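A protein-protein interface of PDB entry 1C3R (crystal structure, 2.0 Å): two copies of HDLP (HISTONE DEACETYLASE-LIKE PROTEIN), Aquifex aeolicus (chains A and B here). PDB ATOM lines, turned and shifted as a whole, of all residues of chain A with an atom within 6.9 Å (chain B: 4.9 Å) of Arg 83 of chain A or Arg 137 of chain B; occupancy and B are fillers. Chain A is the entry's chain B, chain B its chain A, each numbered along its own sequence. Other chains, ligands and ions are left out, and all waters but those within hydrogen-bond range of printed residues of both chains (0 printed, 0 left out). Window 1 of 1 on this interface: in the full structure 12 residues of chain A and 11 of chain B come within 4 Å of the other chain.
The side-chain carboxylate (OE2) of Glu 201 of chain B is in salt-bridge range of the guanidinium group (NH2) of Arg 83 of chain A, 2.8 Å away.
O of Glu 84 of chain A lies close to O of Glu 84 of chain B.
O of Glu 84 of chain B is in hydrogen-bond range of NH2 of Arg 137 of chain B (2.9 Å).
The backbone carbonyl oxygen of Glu 84 of chain A is in hydrogen-bond range of the guanidinium group of Arg 137 of chain A (3.0 Å).
Printed residues of chain A within 4 Å of Arg 137 of chain B: Arg 83 (3.9 Å) and Glu 84 (3.97 Å).
Of the printed residues of chain B, Glu 84 of chain A touches Glu 84 (3.3 Å) and Arg 137 (3.97 Å).
Of the printed residues of chain A, Glu 84 of chain B touches Glu 84.
Printed residues of chain B within 4 Å of Gly 89 of chain A: Glu 201.
Printed residues of chain B within 4 Å of Arg 137 of chain A: Arg 83 (3.8 Å).
Printed residues of chain B within 4 Å of Tyr 91 of chain A: Glu 201 (3.5 Å).
Lys 80 of chain A touches none of the printed residues of chain B.
The nearest printed residue of chain A that does not touch Arg 137 of chain B is Arg 137 of chain A (4.01 Å).
The nearest printed residue of chain A that does not touch Arg 83 of chain B is Glu 84 of chain A (6.1 Å).
Of the 16 printed residues of chain A, 6 touch a printed residue of chain B.
Hydrophobic or aromatic side chains of chain A that line the printed part of chain B: Tyr 91.
Of the 15 printed residues of chain B, 4 touch a printed residue of chain A.
Among the printed residues, Asp or Glu carboxylates within 4 Å of a Lys or Arg side-chain nitrogen of the other chain: Arg 83 of chain A with Glu 201 of chain B (2.8 Å).
Among the printed residues, pairs that only touch across the chains: Tyr 91 of chain A with Glu 201 of chain B (3.5 Å), Gly 90 of chain A with Glu 201 of chain B (3.6 Å), Arg 137 of chain A with Arg 83 of chain B (3.8 Å), Arg 83 of chain A with Arg 137 of chain B (3.9 Å), Glu 84 of chain A with Arg 137 of chain B (3.97 Å) and Gly 89 of chain A with Glu 201 of chain B (3.97 Å).
Arg 83 of chain A touches Arg 137 of chain B, and with the chains exchanged Arg 137 of chain A touches Arg 83 of chain B.
Glu 84 of chain A touches its own counterpart, Glu 84 of chain B.
Glu 84 of chain A touches Arg 137 of chain B, but with the chains exchanged Arg 137 of chain A does not touch Glu 84 of chain B (4.1 Å).
Positions printed for both chains: 83, 84, 85, 86, 87 and 137.
Of the 8 pairs that touch across the chains among the printed residues, 3 have their exchanged pair printed and touching as well.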
ATOM      1  N   THR A  68      -5.695   1.744  23.290  1.00  0.00           N
ATOM      2  CA  THR A  68      -7.064   1.283  23.086  1.00  0.00           C
ATOM      3  C   THR A  68      -7.707   0.908  24.414  1.00  0.00           C
ATOM      4  O   THR A  68      -8.868   1.236  24.652  1.00  0.00           O
ATOM      5  CB  THR A  68      -7.123   0.083  22.130  1.00  0.00           C
ATOM      6  OG1 THR A  68      -6.701   0.502  20.823  1.00  0.00           O
ATOM      7  CG2 THR A  68      -8.545  -0.474  22.049  1.00  0.00           C
ATOM      8  N   VAL A  78     -16.535   0.215  23.492  1.00  0.00           N
ATOM      9  CA  VAL A  78     -15.584  -0.442  22.617  1.00  0.00           C
ATOM     10  C   VAL A  78     -15.322   0.377  21.365  1.00  0.00           C
ATOM     11  O   VAL A  78     -16.190   0.508  20.501  1.00  0.00           O
ATOM     12  CB  VAL A  78     -16.090  -1.822  22.179  1.00  0.00           C
ATOM     13  CG1 VAL A  78     -15.061  -2.483  21.263  1.00  0.00           C
ATOM     14  CG2 VAL A  78     -16.366  -2.682  23.402  1.00  0.00           C
ATOM     15  N   PRO A  79     -14.113   0.945  21.251  1.00  0.00           N
ATOM     16  CA  PRO A  79     -13.731   1.754  20.093  1.00  0.00           C
ATOM     17  C   PRO A  79     -13.914   0.995  18.779  1.00  0.00           C
ATOM     18  O   PRO A  79     -13.804  -0.228  18.734  1.00  0.00           O
ATOM     19  CB  PRO A  79     -12.268   2.078  20.390  1.00  0.00           C
ATOM     20  CG  PRO A  79     -12.274   2.168  21.905  1.00  0.00           C
ATOM     21  CD  PRO A  79     -12.997   0.881  22.208  1.00  0.00           C
ATOM     22  N   LYS A  80     -14.200   1.737  17.716  1.00  0.00           N
ATOM     23  CA  LYS A  80     -14.409   1.181  16.381  1.00  0.00           C
ATOM     24  C   LYS A  80     -13.396   0.100  16.000  1.00  0.00           C
ATOM     25  O   LYS A  80     -12.190   0.332  16.015  1.00  0.00           O
ATOM     26  CB  LYS A  80     -14.351   2.316  15.351  1.00  0.00           C
ATOM     27  CG  LYS A  80     -14.520   1.904  13.890  1.00  0.00           C
ATOM     28  CD  LYS A  80     -14.300   3.113  12.977  1.00  0.00           C
ATOM     29  CE  LYS A  80     -14.470   2.774  11.507  1.00  0.00           C
ATOM     30  NZ  LYS A  80     -15.873   2.378  11.190  1.00  0.00           N
ATOM     31  N   GLY A  81     -13.902  -1.082  15.658  1.00  0.00           N
ATOM     32  CA  GLY A  81     -13.044  -2.177  15.248  1.00  0.00           C
ATOM     33  C   GLY A  81     -12.141  -2.774  16.311  1.00  0.00           C
ATOM     34  O   GLY A  81     -11.458  -3.765  16.058  1.00  0.00           O
ATOM     35  N   ALA A  82     -12.136  -2.186  17.500  1.00  0.00           N
ATOM     36  CA  ALA A  82     -11.295  -2.675  18.586  1.00  0.00           C
ATOM     37  C   ALA A  82     -11.702  -4.073  19.062  1.00  0.00           C
ATOM     38  O   ALA A  82     -10.862  -4.870  19.480  1.00  0.00           O
ATOM     39  CB  ALA A  82     -11.341  -1.699  19.743  1.00  0.00           C
ATOM     40  N   ARG A  83     -12.994  -4.367  18.996  1.00  0.00           N
ATOM     41  CA  ARG A  83     -13.506  -5.655  19.441  1.00  0.00           C
ATOM     42  C   ARG A  83     -12.843  -6.816  18.717  1.00  0.00           C
ATOM     43  O   ARG A  83     -12.429  -7.794  19.336  1.00  0.00           O
ATOM     44  CB  ARG A  83     -15.014  -5.715  19.224  1.00  0.00           C
ATOM     45  CG  ARG A  83     -15.660  -6.932  19.827  1.00  0.00           C
ATOM     46  CD  ARG A  83     -17.154  -6.970  19.558  1.00  0.00           C
ATOM     47  NE  ARG A  83     -17.842  -7.962  20.386  1.00  0.00           N
ATOM     48  CZ  ARG A  83     -17.503  -9.247  20.479  1.00  0.00           C
ATOM     49  NH1 ARG A  83     -16.470  -9.726  19.796  1.00  0.00           N
ATOM     50  NH2 ARG A  83     -18.206 -10.059  21.258  1.00  0.00           N
ATOM     51  N   GLU A  84     -12.742  -6.702  17.399  1.00  0.00           N
ATOM     52  CA  GLU A  84     -12.137  -7.742  16.578  1.00  0.00           C
ATOM     53  C   GLU A  84     -10.618  -7.648  16.466  1.00  0.00           C
ATOM     54  O   GLU A  84      -9.935  -8.656  16.287  1.00  0.00           O
ATOM     55  CB  GLU A  84     -12.754  -7.720  15.176  1.00  0.00           C
ATOM     56  CG  GLU A  84     -13.216  -6.345  14.760  1.00  0.00           C
ATOM     57  CD  GLU A  84     -14.481  -5.937  15.494  1.00  0.00           C
ATOM     58  OE1 GLU A  84     -14.721  -4.722  15.644  1.00  0.00           O
ATOM     59  OE2 GLU A  84     -15.244  -6.841  15.906  1.00  0.00           O
ATOM     60  N   LYS A  85     -10.082  -6.441  16.560  1.00  0.00           N
ATOM     61  CA  LYS A  85      -8.639  -6.276  16.446  1.00  0.00           C
ATOM     62  C   LYS A  85      -7.926  -6.502  17.775  1.00  0.00           C
ATOM     63  O   LYS A  85      -6.822  -7.039  17.810  1.00  0.00           O
ATOM     64  CB  LYS A  85      -8.307  -4.877  15.924  1.00  0.00           C
ATOM     65  CG  LYS A  85      -6.817  -4.615  15.749  1.00  0.00           C
ATOM     66  CD  LYS A  85      -6.564  -3.203  15.212  1.00  0.00           C
ATOM     67  CE  LYS A  85      -5.077  -2.942  15.035  1.00  0.00           C
ATOM     68  NZ  LYS A  85      -4.796  -1.550  14.598  1.00  0.00           N
ATOM     69  N   TYR A  86      -8.573  -6.108  18.864  1.00  0.00           N
ATOM     70  CA  TYR A  86      -7.982  -6.224  20.189  1.00  0.00           C
ATOM     71  C   TYR A  86      -8.679  -7.233  21.106  1.00  0.00           C
ATOM     72  O   TYR A  86      -8.264  -7.444  22.245  1.00  0.00           O
ATOM     73  CB  TYR A  86      -7.953  -4.829  20.825  1.00  0.00           C
ATOM     74  CG  TYR A  86      -7.109  -3.838  20.036  1.00  0.00           C
ATOM     75  CD1 TYR A  86      -5.726  -3.996  19.942  1.00  0.00           C
ATOM     76  CD2 TYR A  86      -7.694  -2.754  19.378  1.00  0.00           C
ATOM     77  CE1 TYR A  86      -4.939  -3.103  19.219  1.00  0.00           C
ATOM     78  CE2 TYR A  86      -6.912  -1.846  18.644  1.00  0.00           C
ATOM     79  CZ  TYR A  86      -5.534  -2.030  18.573  1.00  0.00           C
ATOM     80  OH  TYR A  86      -4.746  -1.144  17.870  1.00  0.00           O
ATOM     81  N   ASN A  87      -9.743  -7.847  20.604  1.00  0.00           N
ATOM     82  CA  ASN A  87     -10.481  -8.867  21.346  1.00  0.00           C
ATOM     83  C   ASN A  87     -11.040  -8.408  22.691  1.00  0.00           C
ATOM     84  O   ASN A  87     -11.083  -9.173  23.659  1.00  0.00           O
ATOM     85  CB  ASN A  87      -9.587 -10.091  21.549  1.00  0.00           C
ATOM     86  CG  ASN A  87     -10.364 -11.310  21.984  1.00  0.00           C
ATOM     87  OD1 ASN A  87     -11.388 -11.648  21.388  1.00  0.00           O
ATOM     88  ND2 ASN A  87      -9.873 -11.993  23.010  1.00  0.00           N
ATOM     89  N   ILE A  88     -11.466  -7.151  22.732  1.00  0.00           N
ATOM     90  CA  ILE A  88     -12.056  -6.551  23.917  1.00  0.00           C
ATOM     91  C   ILE A  88     -13.536  -6.253  23.660  1.00  0.00           C
ATOM     92  O   ILE A  88     -13.925  -5.965  22.529  1.00  0.00           O
ATOM     93  CB  ILE A  88     -11.370  -5.222  24.244  1.00  0.00           C
ATOM     94  CG1 ILE A  88      -9.916  -5.456  24.624  1.00  0.00           C
ATOM     95  CG2 ILE A  88     -12.108  -4.519  25.368  1.00  0.00           C
ATOM     96  CD1 ILE A  88      -9.765  -6.204  25.901  1.00  0.00           C
ATOM     97  N   GLY A  89     -14.352  -6.309  24.711  1.00  0.00           N
ATOM     98  CA  GLY A  89     -15.771  -6.017  24.563  1.00  0.00           C
ATOM     99  C   GLY A  89     -16.705  -7.213  24.606  1.00  0.00           C
ATOM    100  O   GLY A  89     -17.912  -7.058  24.816  1.00  0.00           O
ATOM    101  N   GLY A  90     -16.159  -8.406  24.388  1.00  0.00           N
ATOM    102  CA  GLY A  90     -16.977  -9.605  24.416  1.00  0.00           C
ATOM    103  C   GLY A  90     -17.203 -10.044  25.851  1.00  0.00           C
ATOM    104  O   GLY A  90     -16.879  -9.308  26.783  1.00  0.00           O
ATOM    105  N   TYR A  91     -17.746 -11.241  26.042  1.00  0.00           N
ATOM    106  CA  TYR A  91     -18.012 -11.735  27.387  1.00  0.00           C
ATOM    107  C   TYR A  91     -16.724 -12.122  28.102  1.00  0.00           C
ATOM    108  O   TYR A  91     -16.650 -12.091  29.326  1.00  0.00           O
ATOM    109  CB  TYR A  91     -18.946 -12.947  27.320  1.00  0.00           C
ATOM    110  CG  TYR A  91     -18.334 -14.161  26.660  1.00  0.00           C
ATOM    111  CD1 TYR A  91     -17.485 -15.014  27.370  1.00  0.00           C
ATOM    112  CD2 TYR A  91     -18.576 -14.442  25.317  1.00  0.00           C
ATOM    113  CE1 TYR A  91     -16.898 -16.114  26.757  1.00  0.00           C
ATOM    114  CE2 TYR A  91     -17.993 -15.535  24.695  1.00  0.00           C
ATOM    115  CZ  TYR A  91     -17.158 -16.367  25.417  1.00  0.00           C
ATOM    116  OH  TYR A  91     -16.591 -17.457  24.806  1.00  0.00           O
ATOM    117  N   ARG A 137      -3.239  -8.001  22.242  1.00  0.00           N
ATOM    118  CA  ARG A 137      -4.612  -8.479  22.289  1.00  0.00           C
ATOM    119  C   ARG A 137      -4.990  -9.125  23.620  1.00  0.00           C
ATOM    120  O   ARG A 137      -4.193  -9.840  24.233  1.00  0.00           O
ATOM    121  CB  ARG A 137      -4.839  -9.476  21.147  1.00  0.00           C
ATOM    122  CG  ARG A 137      -6.276  -9.534  20.690  1.00  0.00           C
ATOM    123  CD  ARG A 137      -6.542 -10.630  19.678  1.00  0.00           C
ATOM    124  NE  ARG A 137      -7.869 -10.445  19.087  1.00  0.00           N
ATOM    125  CZ  ARG A 137      -8.547 -11.387  18.446  1.00  0.00           C
ATOM    126  NH1 ARG A 137      -8.032 -12.599  18.307  1.00  0.00           N
ATOM    127  NH2 ARG A 137      -9.744 -11.112  17.943  1.00  0.00           N
ATOM    128  N   TYR B  65     -16.376 -12.302   3.160  1.00  0.00           N
ATOM    129  CA  TYR B  65     -16.373 -13.382   4.138  1.00  0.00           C
ATOM    130  C   TYR B  65     -16.423 -14.729   3.415  1.00  0.00           C
ATOM    131  O   TYR B  65     -15.597 -15.607   3.659  1.00  0.00           O
ATOM    132  CB  TYR B  65     -17.564 -13.223   5.093  1.00  0.00           C
ATOM    133  CG  TYR B  65     -17.707 -14.355   6.084  1.00  0.00           C
ATOM    134  CD1 TYR B  65     -16.648 -14.716   6.916  1.00  0.00           C
ATOM    135  CD2 TYR B  65     -18.900 -15.072   6.184  1.00  0.00           C
ATOM    136  CE1 TYR B  65     -16.771 -15.767   7.821  1.00  0.00           C
ATOM    137  CE2 TYR B  65     -19.034 -16.129   7.091  1.00  0.00           C
ATOM    138  CZ  TYR B  65     -17.967 -16.472   7.903  1.00  0.00           C
ATOM    139  OH  TYR B  65     -18.091 -17.527   8.788  1.00  0.00           O
ATOM    140  N   ARG B  83      -8.072 -14.283  10.759  1.00  0.00           N
ATOM    141  CA  ARG B  83      -8.350 -14.832  12.083  1.00  0.00           C
ATOM    142  C   ARG B  83      -9.085 -13.834  12.976  1.00  0.00           C
ATOM    143  O   ARG B  83     -10.075 -14.176  13.621  1.00  0.00           O
ATOM    144  CB  ARG B  83      -7.048 -15.252  12.760  1.00  0.00           C
ATOM    145  CG  ARG B  83      -7.257 -16.036  14.030  1.00  0.00           C
ATOM    146  CD  ARG B  83      -5.939 -16.326  14.721  1.00  0.00           C
ATOM    147  NE  ARG B  83      -6.085 -17.306  15.798  1.00  0.00           N
ATOM    148  CZ  ARG B  83      -6.932 -17.200  16.819  1.00  0.00           C
ATOM    149  NH1 ARG B  83      -7.733 -16.145  16.923  1.00  0.00           N
ATOM    150  NH2 ARG B  83      -6.974 -18.154  17.739  1.00  0.00           N
ATOM    151  N   GLU B  84      -8.593 -12.599  13.010  1.00  0.00           N
ATOM    152  CA  GLU B  84      -9.200 -11.552  13.823  1.00  0.00           C
ATOM    153  C   GLU B  84     -10.376 -10.849  13.158  1.00  0.00           C
ATOM    154  O   GLU B  84     -11.295 -10.391  13.836  1.00  0.00           O
ATOM    155  CB  GLU B  84      -8.142 -10.515  14.211  1.00  0.00           C
ATOM    156  CG  GLU B  84      -7.030 -10.391  13.192  1.00  0.00           C
ATOM    157  CD  GLU B  84      -6.101 -11.591  13.230  1.00  0.00           C
ATOM    158  OE1 GLU B  84      -5.447 -11.871  12.204  1.00  0.00           O
ATOM    159  OE2 GLU B  84      -6.012 -12.240  14.295  1.00  0.00           O
ATOM    160  N   LYS B  85     -10.353 -10.759  11.836  1.00  0.00           N
ATOM    161  CA  LYS B  85     -11.434 -10.084  11.128  1.00  0.00           C
ATOM    162  C   LYS B  85     -12.635 -10.993  10.895  1.00  0.00           C
ATOM    163  O   LYS B  85     -13.781 -10.549  10.942  1.00  0.00           O
ATOM    164  CB  LYS B  85     -10.936  -9.557   9.782  1.00  0.00           C
ATOM    165  CG  LYS B  85     -11.980  -8.774   8.994  1.00  0.00           C
ATOM    166  CD  LYS B  85     -11.412  -8.262   7.672  1.00  0.00           C
ATOM    167  CE  LYS B  85     -12.465  -7.500   6.877  1.00  0.00           C
ATOM    168  NZ  LYS B  85     -11.953  -7.060   5.547  1.00  0.00           N
ATOM    169  N   TYR B  86     -12.367 -12.271  10.660  1.00  0.00           N
ATOM    170  CA  TYR B  86     -13.425 -13.224  10.367  1.00  0.00           C
ATOM    171  C   TYR B  86     -13.633 -14.291  11.444  1.00  0.00           C
ATOM    172  O   TYR B  86     -14.520 -15.140  11.334  1.00  0.00           O
ATOM    173  CB  TYR B  86     -13.137 -13.857   9.004  1.00  0.00           C
ATOM    174  CG  TYR B  86     -13.122 -12.846   7.870  1.00  0.00           C
ATOM    175  CD1 TYR B  86     -14.287 -12.180   7.496  1.00  0.00           C
ATOM    176  CD2 TYR B  86     -11.946 -12.552   7.176  1.00  0.00           C
ATOM    177  CE1 TYR B  86     -14.291 -11.254   6.464  1.00  0.00           C
ATOM    178  CE2 TYR B  86     -11.938 -11.619   6.134  1.00  0.00           C
ATOM    179  CZ  TYR B  86     -13.118 -10.976   5.787  1.00  0.00           C
ATOM    180  OH  TYR B  86     -13.142 -10.051   4.774  1.00  0.00           O
ATOM    181  N   ASN B  87     -12.805 -14.241  12.479  1.00  0.00           N
ATOM    182  CA  ASN B  87     -12.893 -15.156  13.609  1.00  0.00           C
ATOM    183  C   ASN B  87     -12.761 -16.631  13.249  1.00  0.00           C
ATOM    184  O   ASN B  87     -13.399 -17.497  13.856  1.00  0.00           O
ATOM    185  CB  ASN B  87     -14.204 -14.907  14.356  1.00  0.00           C
ATOM    186  CG  ASN B  87     -14.240 -15.584  15.699  1.00  0.00           C
ATOM    187  OD1 ASN B  87     -13.300 -15.474  16.479  1.00  0.00           O
ATOM    188  ND2 ASN B  87     -15.332 -16.275  15.986  1.00  0.00           N
ATOM    189  N   ALA B 133     -23.481 -18.119  13.233  1.00  0.00           N
ATOM    190  CA  ALA B 133     -22.730 -17.283  12.297  1.00  0.00           C
ATOM    191  C   ALA B 133     -23.357 -15.929  12.016  1.00  0.00           C
ATOM    192  O   ALA B 133     -24.579 -15.807  11.927  1.00  0.00           O
ATOM    193  CB  ALA B 133     -22.511 -18.029  10.985  1.00  0.00           C
ATOM    194  N   PHE B 134     -22.515 -14.908  11.893  1.00  0.00           N
ATOM    195  CA  PHE B 134     -22.999 -13.573  11.588  1.00  0.00           C
ATOM    196  C   PHE B 134     -22.763 -13.275  10.112  1.00  0.00           C
ATOM    197  O   PHE B 134     -22.113 -14.037   9.398  1.00  0.00           O
ATOM    198  CB  PHE B 134     -22.288 -12.506  12.429  1.00  0.00           C
ATOM    199  CG  PHE B 134     -22.498 -12.648  13.908  1.00  0.00           C
ATOM    200  CD1 PHE B 134     -21.499 -13.186  14.718  1.00  0.00           C
ATOM    201  CD2 PHE B 134     -23.695 -12.248  14.496  1.00  0.00           C
ATOM    202  CE1 PHE B 134     -21.687 -13.323  16.094  1.00  0.00           C
ATOM    203  CE2 PHE B 134     -23.897 -12.381  15.878  1.00  0.00           C
ATOM    204  CZ  PHE B 134     -22.892 -12.917  16.677  1.00  0.00           C
ATOM    205  N   LYS B 135     -23.312 -12.157   9.669  1.00  0.00           N
ATOM    206  CA  LYS B 135     -23.172 -11.703   8.295  1.00  0.00           C
ATOM    207  C   LYS B 135     -21.757 -11.890   7.732  1.00  0.00           C
ATOM    208  O   LYS B 135     -21.580 -12.442   6.645  1.00  0.00           O
ATOM    209  CB  LYS B 135     -23.572 -10.229   8.252  1.00  0.00           C
ATOM    210  CG  LYS B 135     -23.087  -9.444   7.061  1.00  0.00           C
ATOM    211  CD  LYS B 135     -23.507  -7.987   7.216  1.00  0.00           C
ATOM    212  CE  LYS B 135     -22.820  -7.097   6.195  1.00  0.00           C
ATOM    213  NZ  LYS B 135     -21.338  -7.102   6.397  1.00  0.00           N
ATOM    214  N   SER B 136     -20.753 -11.448   8.481  1.00  0.00           N
ATOM    215  CA  SER B 136     -19.373 -11.529   8.010  1.00  0.00           C
ATOM    216  C   SER B 136     -18.392 -12.138   9.004  1.00  0.00           C
ATOM    217  O   SER B 136     -17.212 -11.775   9.001  1.00  0.00           O
ATOM    218  CB  SER B 136     -18.884 -10.124   7.649  1.00  0.00           C
ATOM    219  OG  SER B 136     -19.785  -9.485   6.759  1.00  0.00           O
ATOM    220  N   ARG B 137     -18.849 -13.057   9.847  1.00  0.00           N
ATOM    221  CA  ARG B 137     -17.931 -13.634  10.814  1.00  0.00           C
ATOM    222  C   ARG B 137     -18.415 -14.962  11.384  1.00  0.00           C
ATOM    223  O   ARG B 137     -19.611 -15.152  11.631  1.00  0.00           O
ATOM    224  CB  ARG B 137     -17.705 -12.636  11.952  1.00  0.00           C
ATOM    225  CG  ARG B 137     -16.373 -12.820  12.639  1.00  0.00           C
ATOM    226  CD  ARG B 137     -16.204 -11.937  13.866  1.00  0.00           C
ATOM    227  NE  ARG B 137     -14.807 -11.946  14.295  1.00  0.00           N
ATOM    228  CZ  ARG B 137     -14.382 -11.583  15.497  1.00  0.00           C
ATOM    229  NH1 ARG B 137     -15.250 -11.176  16.413  1.00  0.00           N
ATOM    230  NH2 ARG B 137     -13.087 -11.626  15.782  1.00  0.00           N
ATOM    231  N   ALA B 138     -17.478 -15.881  11.587  1.00  0.00           N
ATOM    232  CA  ALA B 138     -17.804 -17.187  12.140  1.00  0.00           C
ATOM    233  C   ALA B 138     -18.051 -17.024  13.629  1.00  0.00           C
ATOM    234  O   ALA B 138     -17.506 -16.117  14.251  1.00  0.00           O
ATOM    235  CB  ALA B 138     -16.661 -18.152  11.909  1.00  0.00           C
ATOM    236  N   ASN B 139     -18.861 -17.909  14.200  1.00  0.00           N
ATOM    237  CA  ASN B 139     -19.176 -17.831  15.619  1.00  0.00           C
ATOM    238  C   ASN B 139     -19.788 -19.128  16.137  1.00  0.00           C
ATOM    239  O   ASN B 139     -20.574 -19.786  15.445  1.00  0.00           O
ATOM    240  CB  ASN B 139     -20.121 -16.642  15.863  1.00  0.00           C
ATOM    241  CG  ASN B 139     -20.524 -16.494  17.318  1.00  0.00           C
ATOM    242  OD1 ASN B 139     -19.685 -16.565  18.204  1.00  0.00           O
ATOM    243  ND2 ASN B 139     -21.813 -16.262  17.565  1.00  0.00           N
ATOM    244  N   CYS B 142     -20.094 -22.192  14.076  1.00  0.00           N
ATOM    245  CA  CYS B 142     -20.799 -21.950  12.821  1.00  0.00           C
ATOM    246  C   CYS B 142     -20.068 -21.021  11.856  1.00  0.00           C
ATOM    247  O   CYS B 142     -19.633 -19.933  12.233  1.00  0.00           O
ATOM    248  CB  CYS B 142     -22.187 -21.369  13.111  1.00  0.00           C
ATOM    249  SG  CYS B 142     -23.264 -22.438  14.121  1.00  0.00           S
ATOM    250  N   GLU B 201     -23.210 -13.070  25.840  1.00  0.00           N
ATOM    251  CA  GLU B 201     -23.535 -11.673  25.549  1.00  0.00           C
ATOM    252  C   GLU B 201     -24.961 -11.388  25.099  1.00  0.00           C
ATOM    253  O   GLU B 201     -25.431 -10.253  25.181  1.00  0.00           O
ATOM    254  CB  GLU B 201     -22.598 -11.146  24.466  1.00  0.00           C
ATOM    255  CG  GLU B 201     -21.139 -11.348  24.756  1.00  0.00           C
ATOM    256  CD  GLU B 201     -20.284 -10.933  23.586  1.00  0.00           C
ATOM    257  OE1 GLU B 201     -20.353  -9.747  23.203  1.00  0.00           O
ATOM    258  OE2 GLU B 201     -19.554 -11.792  23.051  1.00  0.00           O
